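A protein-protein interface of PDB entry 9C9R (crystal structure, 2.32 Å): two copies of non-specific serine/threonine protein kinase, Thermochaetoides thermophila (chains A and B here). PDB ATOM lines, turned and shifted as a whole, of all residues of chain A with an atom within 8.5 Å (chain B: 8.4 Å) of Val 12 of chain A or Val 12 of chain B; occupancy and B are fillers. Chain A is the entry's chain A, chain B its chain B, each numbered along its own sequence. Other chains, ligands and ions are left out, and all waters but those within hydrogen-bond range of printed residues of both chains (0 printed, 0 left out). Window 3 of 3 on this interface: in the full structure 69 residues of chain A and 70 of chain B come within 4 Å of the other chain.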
ATOM      1  N   SER A   6      20.121 -16.935  15.978  1.00  0.00           N
ATOM      2  CA  SER A   6      20.248 -15.951  14.909  1.00  0.00           C
ATOM      3  C   SER A   6      20.514 -14.571  15.508  1.00  0.00           C
ATOM      4  O   SER A   6      20.468 -14.392  16.728  1.00  0.00           O
ATOM      5  CB  SER A   6      18.978 -15.956  14.051  1.00  0.00           C
ATOM      6  OG  SER A   6      17.825 -15.623  14.810  1.00  0.00           O
ATOM      7  N   PRO A   7      20.822 -13.563  14.675  1.00  0.00           N
ATOM      8  CA  PRO A   7      20.853 -12.186  15.204  1.00  0.00           C
ATOM      9  C   PRO A   7      19.515 -11.750  15.780  1.00  0.00           C
ATOM     10  O   PRO A   7      19.480 -10.882  16.665  1.00  0.00           O
ATOM     11  CB  PRO A   7      21.249 -11.345  13.981  1.00  0.00           C
ATOM     12  CG  PRO A   7      21.958 -12.285  13.080  1.00  0.00           C
ATOM     13  CD  PRO A   7      21.271 -13.615  13.270  1.00  0.00           C
ATOM     14  N   TYR A   8      18.412 -12.333  15.300  1.00  0.00           N
ATOM     15  CA  TYR A   8      17.120 -12.152  15.955  1.00  0.00           C
ATOM     16  C   TYR A   8      17.195 -12.568  17.420  1.00  0.00           C
ATOM     17  O   TYR A   8      16.973 -11.752  18.322  1.00  0.00           O
ATOM     18  CB  TYR A   8      16.039 -12.954  15.228  1.00  0.00           C
ATOM     19  N   PHE A   9      17.542 -13.838  17.673  1.00  0.00           N
ATOM     20  CA  PHE A   9      17.498 -14.378  19.033  1.00  0.00           C
ATOM     21  C   PHE A   9      18.307 -13.543  20.020  1.00  0.00           C
ATOM     22  O   PHE A   9      17.904 -13.398  21.178  1.00  0.00           O
ATOM     23  CB  PHE A   9      17.985 -15.832  19.046  1.00  0.00           C
ATOM     24  N   GLU A  10      19.428 -12.962  19.593  1.00  0.00           N
ATOM     25  CA  GLU A  10      20.305 -12.313  20.561  1.00  0.00           C
ATOM     26  C   GLU A  10      19.913 -10.867  20.872  1.00  0.00           C
ATOM     27  O   GLU A  10      20.154 -10.395  21.990  1.00  0.00           O
ATOM     28  CB  GLU A  10      21.739 -12.385  20.063  1.00  0.00           C
ATOM     29  CG  GLU A  10      22.609 -11.271  20.574  1.00  0.00           C
ATOM     30  CD  GLU A  10      24.013 -11.730  20.811  1.00  0.00           C
ATOM     31  OE1 GLU A  10      24.301 -12.905  20.506  1.00  0.00           O
ATOM     32  OE2 GLU A  10      24.818 -10.917  21.311  1.00  0.00           O
ATOM     33  N   LYS A  11      19.305 -10.151  19.920  1.00  0.00           N
ATOM     34  CA  LYS A  11      18.875  -8.780  20.196  1.00  0.00           C
ATOM     35  C   LYS A  11      17.640  -8.759  21.087  1.00  0.00           C
ATOM     36  O   LYS A  11      17.521  -7.908  21.974  1.00  0.00           O
ATOM     37  CB  LYS A  11      18.602  -8.027  18.890  1.00  0.00           C
ATOM     38  N   VAL A  12      16.701  -9.677  20.860  1.00  0.00           N
ATOM     39  CA  VAL A  12      15.538  -9.756  21.735  1.00  0.00           C
ATOM     40  C   VAL A  12      15.970 -10.124  23.150  1.00  0.00           C
ATOM     41  O   VAL A  12      15.385  -9.654  24.139  1.00  0.00           O
ATOM     42  CB  VAL A  12      14.516 -10.764  21.166  1.00  0.00           C
ATOM     43  CG1 VAL A  12      13.199 -10.672  21.916  1.00  0.00           C
ATOM     44  CG2 VAL A  12      14.293 -10.527  19.672  1.00  0.00           C
ATOM     45  N   LEU A  13      17.020 -10.942  23.263  1.00  0.00           N
ATOM     46  CA  LEU A  13      17.515 -11.393  24.557  1.00  0.00           C
ATOM     47  C   LEU A  13      18.021 -10.223  25.394  1.00  0.00           C
ATOM     48  O   LEU A  13      17.568 -10.013  26.528  1.00  0.00           O
ATOM     49  CB  LEU A  13      18.618 -12.426  24.343  1.00  0.00           C
ATOM     50  CG  LEU A  13      18.884 -13.351  25.519  1.00  0.00           C
ATOM     51  CD1 LEU A  13      17.566 -13.924  25.997  1.00  0.00           C
ATOM     52  CD2 LEU A  13      19.833 -14.456  25.085  1.00  0.00           C
ATOM     53  N   GLY A  14      18.970  -9.447  24.849  1.00  0.00           N
ATOM     54  CA  GLY A  14      19.444  -8.257  25.546  1.00  0.00           C
ATOM     55  C   GLY A  14      18.339  -7.244  25.804  1.00  0.00           C
ATOM     56  O   GLY A  14      18.407  -6.468  26.761  1.00  0.00           O
ATOM     57  N   SER A  15      17.301  -7.254  24.969  1.00  0.00           N
ATOM     58  CA  SER A  15      16.137  -6.412  25.190  1.00  0.00           C
ATOM     59  C   SER A  15      15.261  -6.950  26.311  1.00  0.00           C
ATOM     60  O   SER A  15      14.636  -6.169  27.029  1.00  0.00           O
ATOM     61  CB  SER A  15      15.334  -6.305  23.890  1.00  0.00           C
ATOM     62  OG  SER A  15      14.103  -5.644  24.098  1.00  0.00           O
ATOM     63  N   LEU A  16      15.185  -8.274  26.458  1.00  0.00           N
ATOM     64  CA  LEU A  16      14.440  -8.863  27.567  1.00  0.00           C
ATOM     65  C   LEU A  16      15.047  -8.482  28.916  1.00  0.00           C
ATOM     66  O   LEU A  16      14.323  -8.282  29.898  1.00  0.00           O
ATOM     67  CB  LEU A  16      14.401 -10.381  27.405  1.00  0.00           C
ATOM     68  CG  LEU A  16      13.248 -10.953  26.588  1.00  0.00           C
ATOM     69  CD1 LEU A  16      13.515 -12.405  26.262  1.00  0.00           C
ATOM     70  CD2 LEU A  16      11.945 -10.808  27.343  1.00  0.00           C
ATOM     71  N   PHE A  17      16.375  -8.364  28.977  1.00  0.00           N
ATOM     72  CA  PHE A  17      17.102  -8.104  30.211  1.00  0.00           C
ATOM     73  C   PHE A  17      17.142  -6.635  30.596  1.00  0.00           C
ATOM     74  O   PHE A  17      17.615  -6.319  31.691  1.00  0.00           O
ATOM     75  CB  PHE A  17      18.539  -8.620  30.101  1.00  0.00           C
ATOM     76  CG  PHE A  17      18.689 -10.078  30.444  1.00  0.00           C
ATOM     77  CD1 PHE A  17      18.675 -10.498  31.763  1.00  0.00           C
ATOM     78  CD2 PHE A  17      18.851 -11.030  29.445  1.00  0.00           C
ATOM     79  CE1 PHE A  17      18.820 -11.849  32.083  1.00  0.00           C
ATOM     80  CE2 PHE A  17      18.995 -12.381  29.760  1.00  0.00           C
ATOM     81  CZ  PHE A  17      18.977 -12.789  31.077  1.00  0.00           C
ATOM     82  N   ALA A  18      16.685  -5.738  29.729  1.00  0.00           N
ATOM     83  CA  ALA A  18      16.568  -4.324  30.051  1.00  0.00           C
ATOM     84  C   ALA A  18      15.128  -3.909  30.309  1.00  0.00           C
ATOM     85  O   ALA A  18      14.862  -2.723  30.524  1.00  0.00           O
ATOM     86  CB  ALA A  18      17.160  -3.475  28.920  1.00  0.00           C
ATOM     87  N   ARG A  19      14.194  -4.852  30.291  1.00  0.00           N
ATOM     88  CA  ARG A  19      12.795  -4.521  30.481  1.00  0.00           C
ATOM     89  C   ARG A  19      12.503  -4.344  31.959  1.00  0.00           C
ATOM     90  O   ARG A  19      12.971  -5.119  32.796  1.00  0.00           O
ATOM     91  CB  ARG A  19      11.914  -5.614  29.892  1.00  0.00           C
ATOM     92  CG  ARG A  19      10.487  -5.206  29.664  1.00  0.00           C
ATOM     93  CD  ARG A  19       9.941  -6.015  28.524  1.00  0.00           C
ATOM     94  NE  ARG A  19      10.156  -7.438  28.748  1.00  0.00           N
ATOM     95  CZ  ARG A  19       9.185  -8.334  28.819  1.00  0.00           C
ATOM     96  NH1 ARG A  19       7.921  -7.999  28.613  1.00  0.00           N
ATOM     97  NH2 ARG A  19       9.487  -9.599  29.096  1.00  0.00           N
ATOM     98  N   LEU A  83      16.822 -18.349  32.659  1.00  0.00           N
ATOM     99  CA  LEU A  83      17.625 -17.991  31.495  1.00  0.00           C
ATOM    100  C   LEU A  83      18.713 -17.006  31.907  1.00  0.00           C
ATOM    101  O   LEU A  83      18.416 -15.997  32.555  1.00  0.00           O
ATOM    102  CB  LEU A  83      16.743 -17.351  30.423  1.00  0.00           C
ATOM    103  CG  LEU A  83      16.556 -17.941  29.030  1.00  0.00           C
ATOM    104  CD1 LEU A  83      15.867 -19.322  29.068  1.00  0.00           C
ATOM    105  CD2 LEU A  83      15.752 -16.927  28.189  1.00  0.00           C
ATOM    106  N   GLY A  87      21.575 -16.925  27.052  1.00  0.00           N
ATOM    107  CA  GLY A  87      20.466 -17.743  26.622  1.00  0.00           C
ATOM    108  C   GLY A  87      20.400 -19.150  27.195  1.00  0.00           C
ATOM    109  O   GLY A  87      19.394 -19.826  26.979  1.00  0.00           O
ATOM    110  N   SER B   6       5.089  -6.121  23.449  1.00  0.00           N
ATOM    111  CA  SER B   6       5.547  -6.633  22.157  1.00  0.00           C
ATOM    112  C   SER B   6       5.527  -8.156  22.146  1.00  0.00           C
ATOM    113  O   SER B   6       6.108  -8.783  23.048  1.00  0.00           O
ATOM    114  CB  SER B   6       6.962  -6.133  21.855  1.00  0.00           C
ATOM    115  OG  SER B   6       7.347  -6.352  20.502  1.00  0.00           O
ATOM    116  N   PRO B   7       4.891  -8.781  21.146  1.00  0.00           N
ATOM    117  CA  PRO B   7       4.805 -10.251  21.121  1.00  0.00           C
ATOM    118  C   PRO B   7       6.126 -10.924  20.825  1.00  0.00           C
ATOM    119  O   PRO B   7       6.233 -12.142  21.026  1.00  0.00           O
ATOM    120  CB  PRO B   7       3.793 -10.522  20.003  1.00  0.00           C
ATOM    121  CG  PRO B   7       4.043  -9.403  19.049  1.00  0.00           C
ATOM    122  CD  PRO B   7       4.342  -8.184  19.915  1.00  0.00           C
ATOM    123  N   TYR B   8       7.124 -10.179  20.337  1.00  0.00           N
ATOM    124  CA  TYR B   8       8.466 -10.731  20.230  1.00  0.00           C
ATOM    125  C   TYR B   8       8.969 -11.209  21.587  1.00  0.00           C
ATOM    126  O   TYR B   8       9.764 -12.153  21.656  1.00  0.00           O
ATOM    127  CB  TYR B   8       9.418  -9.691  19.636  1.00  0.00           C
ATOM    128  N   PHE B   9       8.487 -10.603  22.673  1.00  0.00           N
ATOM    129  CA  PHE B   9       8.974 -10.963  24.000  1.00  0.00           C
ATOM    130  C   PHE B   9       8.528 -12.369  24.400  1.00  0.00           C
ATOM    131  O   PHE B   9       9.367 -13.212  24.736  1.00  0.00           O
ATOM    132  CB  PHE B   9       8.534  -9.913  25.021  1.00  0.00           C
ATOM    133  CG  PHE B   9       9.372  -8.680  24.998  1.00  0.00           C
ATOM    134  CD1 PHE B   9      10.728  -8.766  24.737  1.00  0.00           C
ATOM    135  CD2 PHE B   9       8.804  -7.423  25.196  1.00  0.00           C
ATOM    136  CE1 PHE B   9      11.522  -7.623  24.697  1.00  0.00           C
ATOM    137  CE2 PHE B   9       9.591  -6.275  25.153  1.00  0.00           C
ATOM    138  CZ  PHE B   9      10.949  -6.374  24.906  1.00  0.00           C
ATOM    139  N   GLU B  10       7.220 -12.652  24.361  1.00  0.00           N
ATOM    140  CA  GLU B  10       6.779 -14.026  24.585  1.00  0.00           C
ATOM    141  C   GLU B  10       7.509 -14.975  23.654  1.00  0.00           C
ATOM    142  O   GLU B  10       8.161 -15.925  24.095  1.00  0.00           O
ATOM    143  CB  GLU B  10       5.272 -14.177  24.388  1.00  0.00           C
ATOM    144  CG  GLU B  10       4.688 -15.454  25.015  1.00  0.00           C
ATOM    145  CD  GLU B  10       4.610 -16.677  24.067  1.00  0.00           C
ATOM    146  OE1 GLU B  10       5.310 -16.706  23.023  1.00  0.00           O
ATOM    147  OE2 GLU B  10       3.852 -17.617  24.346  1.00  0.00           O
ATOM    148  N   LYS B  11       7.393 -14.721  22.350  1.00  0.00           N
ATOM    149  CA  LYS B  11       7.823 -15.681  21.337  1.00  0.00           C
ATOM    150  C   LYS B  11       9.242 -16.172  21.604  1.00  0.00           C
ATOM    151  O   LYS B  11       9.498 -17.383  21.594  1.00  0.00           O
ATOM    152  CB  LYS B  11       7.722 -15.047  19.942  1.00  0.00           C
ATOM    153  N   VAL B  12      10.163 -15.250  21.900  1.00  0.00           N
ATOM    154  CA  VAL B  12      11.553 -15.615  22.170  1.00  0.00           C
ATOM    155  C   VAL B  12      11.733 -16.234  23.568  1.00  0.00           C
ATOM    156  O   VAL B  12      12.655 -17.037  23.788  1.00  0.00           O
ATOM    157  CB  VAL B  12      12.427 -14.363  21.953  1.00  0.00           C
ATOM    158  CG1 VAL B  12      13.906 -14.630  22.260  1.00  0.00           C
ATOM    159  CG2 VAL B  12      12.259 -13.862  20.527  1.00  0.00           C
ATOM    160  N   LEU B  13      10.872 -15.897  24.533  1.00  0.00           N
ATOM    161  CA  LEU B  13      10.976 -16.549  25.836  1.00  0.00           C
ATOM    162  C   LEU B  13      10.592 -18.018  25.732  1.00  0.00           C
ATOM    163  O   LEU B  13      11.394 -18.906  26.053  1.00  0.00           O
ATOM    164  CB  LEU B  13      10.105 -15.842  26.870  1.00  0.00           C
ATOM    165  CG  LEU B  13      10.740 -14.712  27.679  1.00  0.00           C
ATOM    166  CD1 LEU B  13       9.786 -14.353  28.789  1.00  0.00           C
ATOM    167  CD2 LEU B  13      12.095 -15.103  28.244  1.00  0.00           C
ATOM    168  N   GLY B  14       9.363 -18.289  25.276  1.00  0.00           N
ATOM    169  CA  GLY B  14       8.949 -19.667  25.075  1.00  0.00           C
ATOM    170  C   GLY B  14       9.934 -20.438  24.225  1.00  0.00           C
ATOM    171  O   GLY B  14      10.273 -21.587  24.528  1.00  0.00           O
ATOM    172  N   SER B  15      10.446 -19.800  23.175  1.00  0.00           N
ATOM    173  CA  SER B  15      11.381 -20.476  22.288  1.00  0.00           C
ATOM    174  C   SER B  15      12.683 -20.819  23.011  1.00  0.00           C
ATOM    175  O   SER B  15      13.188 -21.944  22.901  1.00  0.00           O
ATOM    176  CB  SER B  15      11.642 -19.600  21.061  1.00  0.00           C
ATOM    177  OG  SER B  15      12.406 -20.303  20.103  1.00  0.00           O
ATOM    178  N   LEU B  16      13.229 -19.871  23.776  1.00  0.00           N
ATOM    179  CA  LEU B  16      14.527 -20.097  24.399  1.00  0.00           C
ATOM    180  C   LEU B  16      14.451 -21.067  25.573  1.00  0.00           C
ATOM    181  O   LEU B  16      15.413 -21.802  25.819  1.00  0.00           O
ATOM    182  CB  LEU B  16      15.138 -18.767  24.829  1.00  0.00           C
ATOM    183  CG  LEU B  16      16.162 -18.328  23.779  1.00  0.00           C
ATOM    184  CD1 LEU B  16      16.590 -16.895  24.004  1.00  0.00           C
ATOM    185  CD2 LEU B  16      17.366 -19.279  23.771  1.00  0.00           C
ATOM    186  N   PHE B  17      13.322 -21.104  26.286  1.00  0.00           N
ATOM    187  CA  PHE B  17      13.128 -22.092  27.336  1.00  0.00           C
ATOM    188  C   PHE B  17      12.903 -23.493  26.790  1.00  0.00           C
ATOM    189  O   PHE B  17      12.825 -24.445  27.579  1.00  0.00           O
ATOM    190  CB  PHE B  17      11.949 -21.692  28.234  1.00  0.00           C
ATOM    191  CG  PHE B  17      12.336 -20.788  29.360  1.00  0.00           C
ATOM    192  CD1 PHE B  17      13.059 -21.279  30.435  1.00  0.00           C
ATOM    193  CD2 PHE B  17      11.996 -19.442  29.340  1.00  0.00           C
ATOM    194  CE1 PHE B  17      13.432 -20.444  31.483  1.00  0.00           C
ATOM    195  CE2 PHE B  17      12.366 -18.605  30.374  1.00  0.00           C
ATOM    196  CZ  PHE B  17      13.094 -19.104  31.453  1.00  0.00           C
ATOM    197  N   ALA B  18      12.792 -23.638  25.471  1.00  0.00           N
ATOM    198  CA  ALA B  18      12.567 -24.932  24.847  1.00  0.00           C
ATOM    199  C   ALA B  18      13.797 -25.476  24.144  1.00  0.00           C
ATOM    200  O   ALA B  18      13.880 -26.684  23.935  1.00  0.00           O
ATOM    201  CB  ALA B  18      11.414 -24.842  23.846  1.00  0.00           C
ATOM    202  N   ARG B  19      14.746 -24.624  23.768  1.00  0.00           N
ATOM    203  CA  ARG B  19      15.993 -25.129  23.216  1.00  0.00           C
ATOM    204  C   ARG B  19      16.715 -25.968  24.269  1.00  0.00           C
ATOM    205  O   ARG B  19      16.551 -25.768  25.476  1.00  0.00           O
ATOM    206  CB  ARG B  19      16.873 -23.969  22.740  1.00  0.00           C
ATOM    207  N   LEU B  83      16.361 -14.548  34.029  1.00  0.00           N
ATOM    208  CA  LEU B  83      14.970 -14.389  33.633  1.00  0.00           C
ATOM    209  C   LEU B  83      14.183 -15.634  34.010  1.00  0.00           C
ATOM    210  O   LEU B  83      14.604 -16.751  33.708  1.00  0.00           O
ATOM    211  CB  LEU B  83      14.860 -14.171  32.126  1.00  0.00           C
ATOM    212  CG  LEU B  83      15.282 -12.847  31.496  1.00  0.00           C
ATOM    213  CD1 LEU B  83      15.570 -13.036  30.013  1.00  0.00           C
ATOM    214  CD2 LEU B  83      14.169 -11.830  31.689  1.00  0.00           C
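Of the printed residues of chain B, Val 12 of chain A touches Tyr 8 (3.7 Å) and Val 12 (3.6 Å). Val 12 of chain B touches just one residue of chain A: Val 12 (3.6 Å). Printed residues of chain B within 4 Å of Leu 16 of chain A: Phe 9 (3.5 Å), Leu 13 (3.6 Å) and Leu 83 (3.9 Å). Printed residues of chain A within 4 Å of Phe 9 of chain B: Ser 15 (3.3 Å), Leu 16 (3.5 Å) and Arg 19 (3.4 Å). Of the printed residues of chain B, Arg 19 of chain A touches Phe 9 (3.4 Å). Printed residues of chain B within 4 Å of Ser 15 of chain A: Phe 9. Printed residues of chain A within 4 Å of Leu 13 of chain B: Leu 16.
CG1 of Val 12 of chain A touches O of Tyr 8 of chain B, 3.7 Å away. Val 12 of chain A touches Val 12 of chain B (CG1 to CG2, 3.6 Å). Leu 16 of chain B touches Leu 13 of chain A (CD1 to CD1, 3.7 Å). Ser 15 of chain A touches Phe 9 of chain B (OG to CE1, 3.3 Å). Leu 16 of chain A touches Phe 9 of chain B. CD2 of Leu 13 of chain B touches CD1 of Leu 16 of chain A (3.6 Å). Leu 83 of chain B touches Leu 16 of chain A. CE2 of Phe 17 of chain A touches CD1 of Leu 83 of chain B, at 3.5 Å. CD2 of Leu 83 of chain A touches CB of Leu 16 of chain B (3.9 Å). Leu 16 of chain B touches Gly 87 of chain A (CD2 to O, 3.8 Å).
Hydrophobic or aromatic side chains of chain B that line the printed part of chain A: Phe 9, Val 12, Leu 13, Leu 16, Phe 17 and Leu 83. Among the printed residues, 13 pairs touch across the chains.
N of Leu 83 of chain B is in hydrogen-bond range of O of Leu 83 of chain A (2.9 Å).
Leu 13 of chain A touches Leu 16 of chain B, and with the chains exchanged Leu 16 of chain A touches Leu 13 of chain B. Leu 16 of chain A touches Phe 9 of chain B, but with the chains exchanged Phe 9 of chain A does not touch Leu 16 of chain B (4.7 Å). Arg 19 of chain A touches Phe 9 of chain B, but with the chains exchanged Phe 9 of chain A does not touch Arg 19 of chain B (9.0 Å). Leu 83 of chain A touches its own counterpart, Leu 83 of chain B. Positions printed for both chains: 6, 7, 8, 9, 10, 11, 12, 13, 14, 15, 16, 17, 18, 19 and 83.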
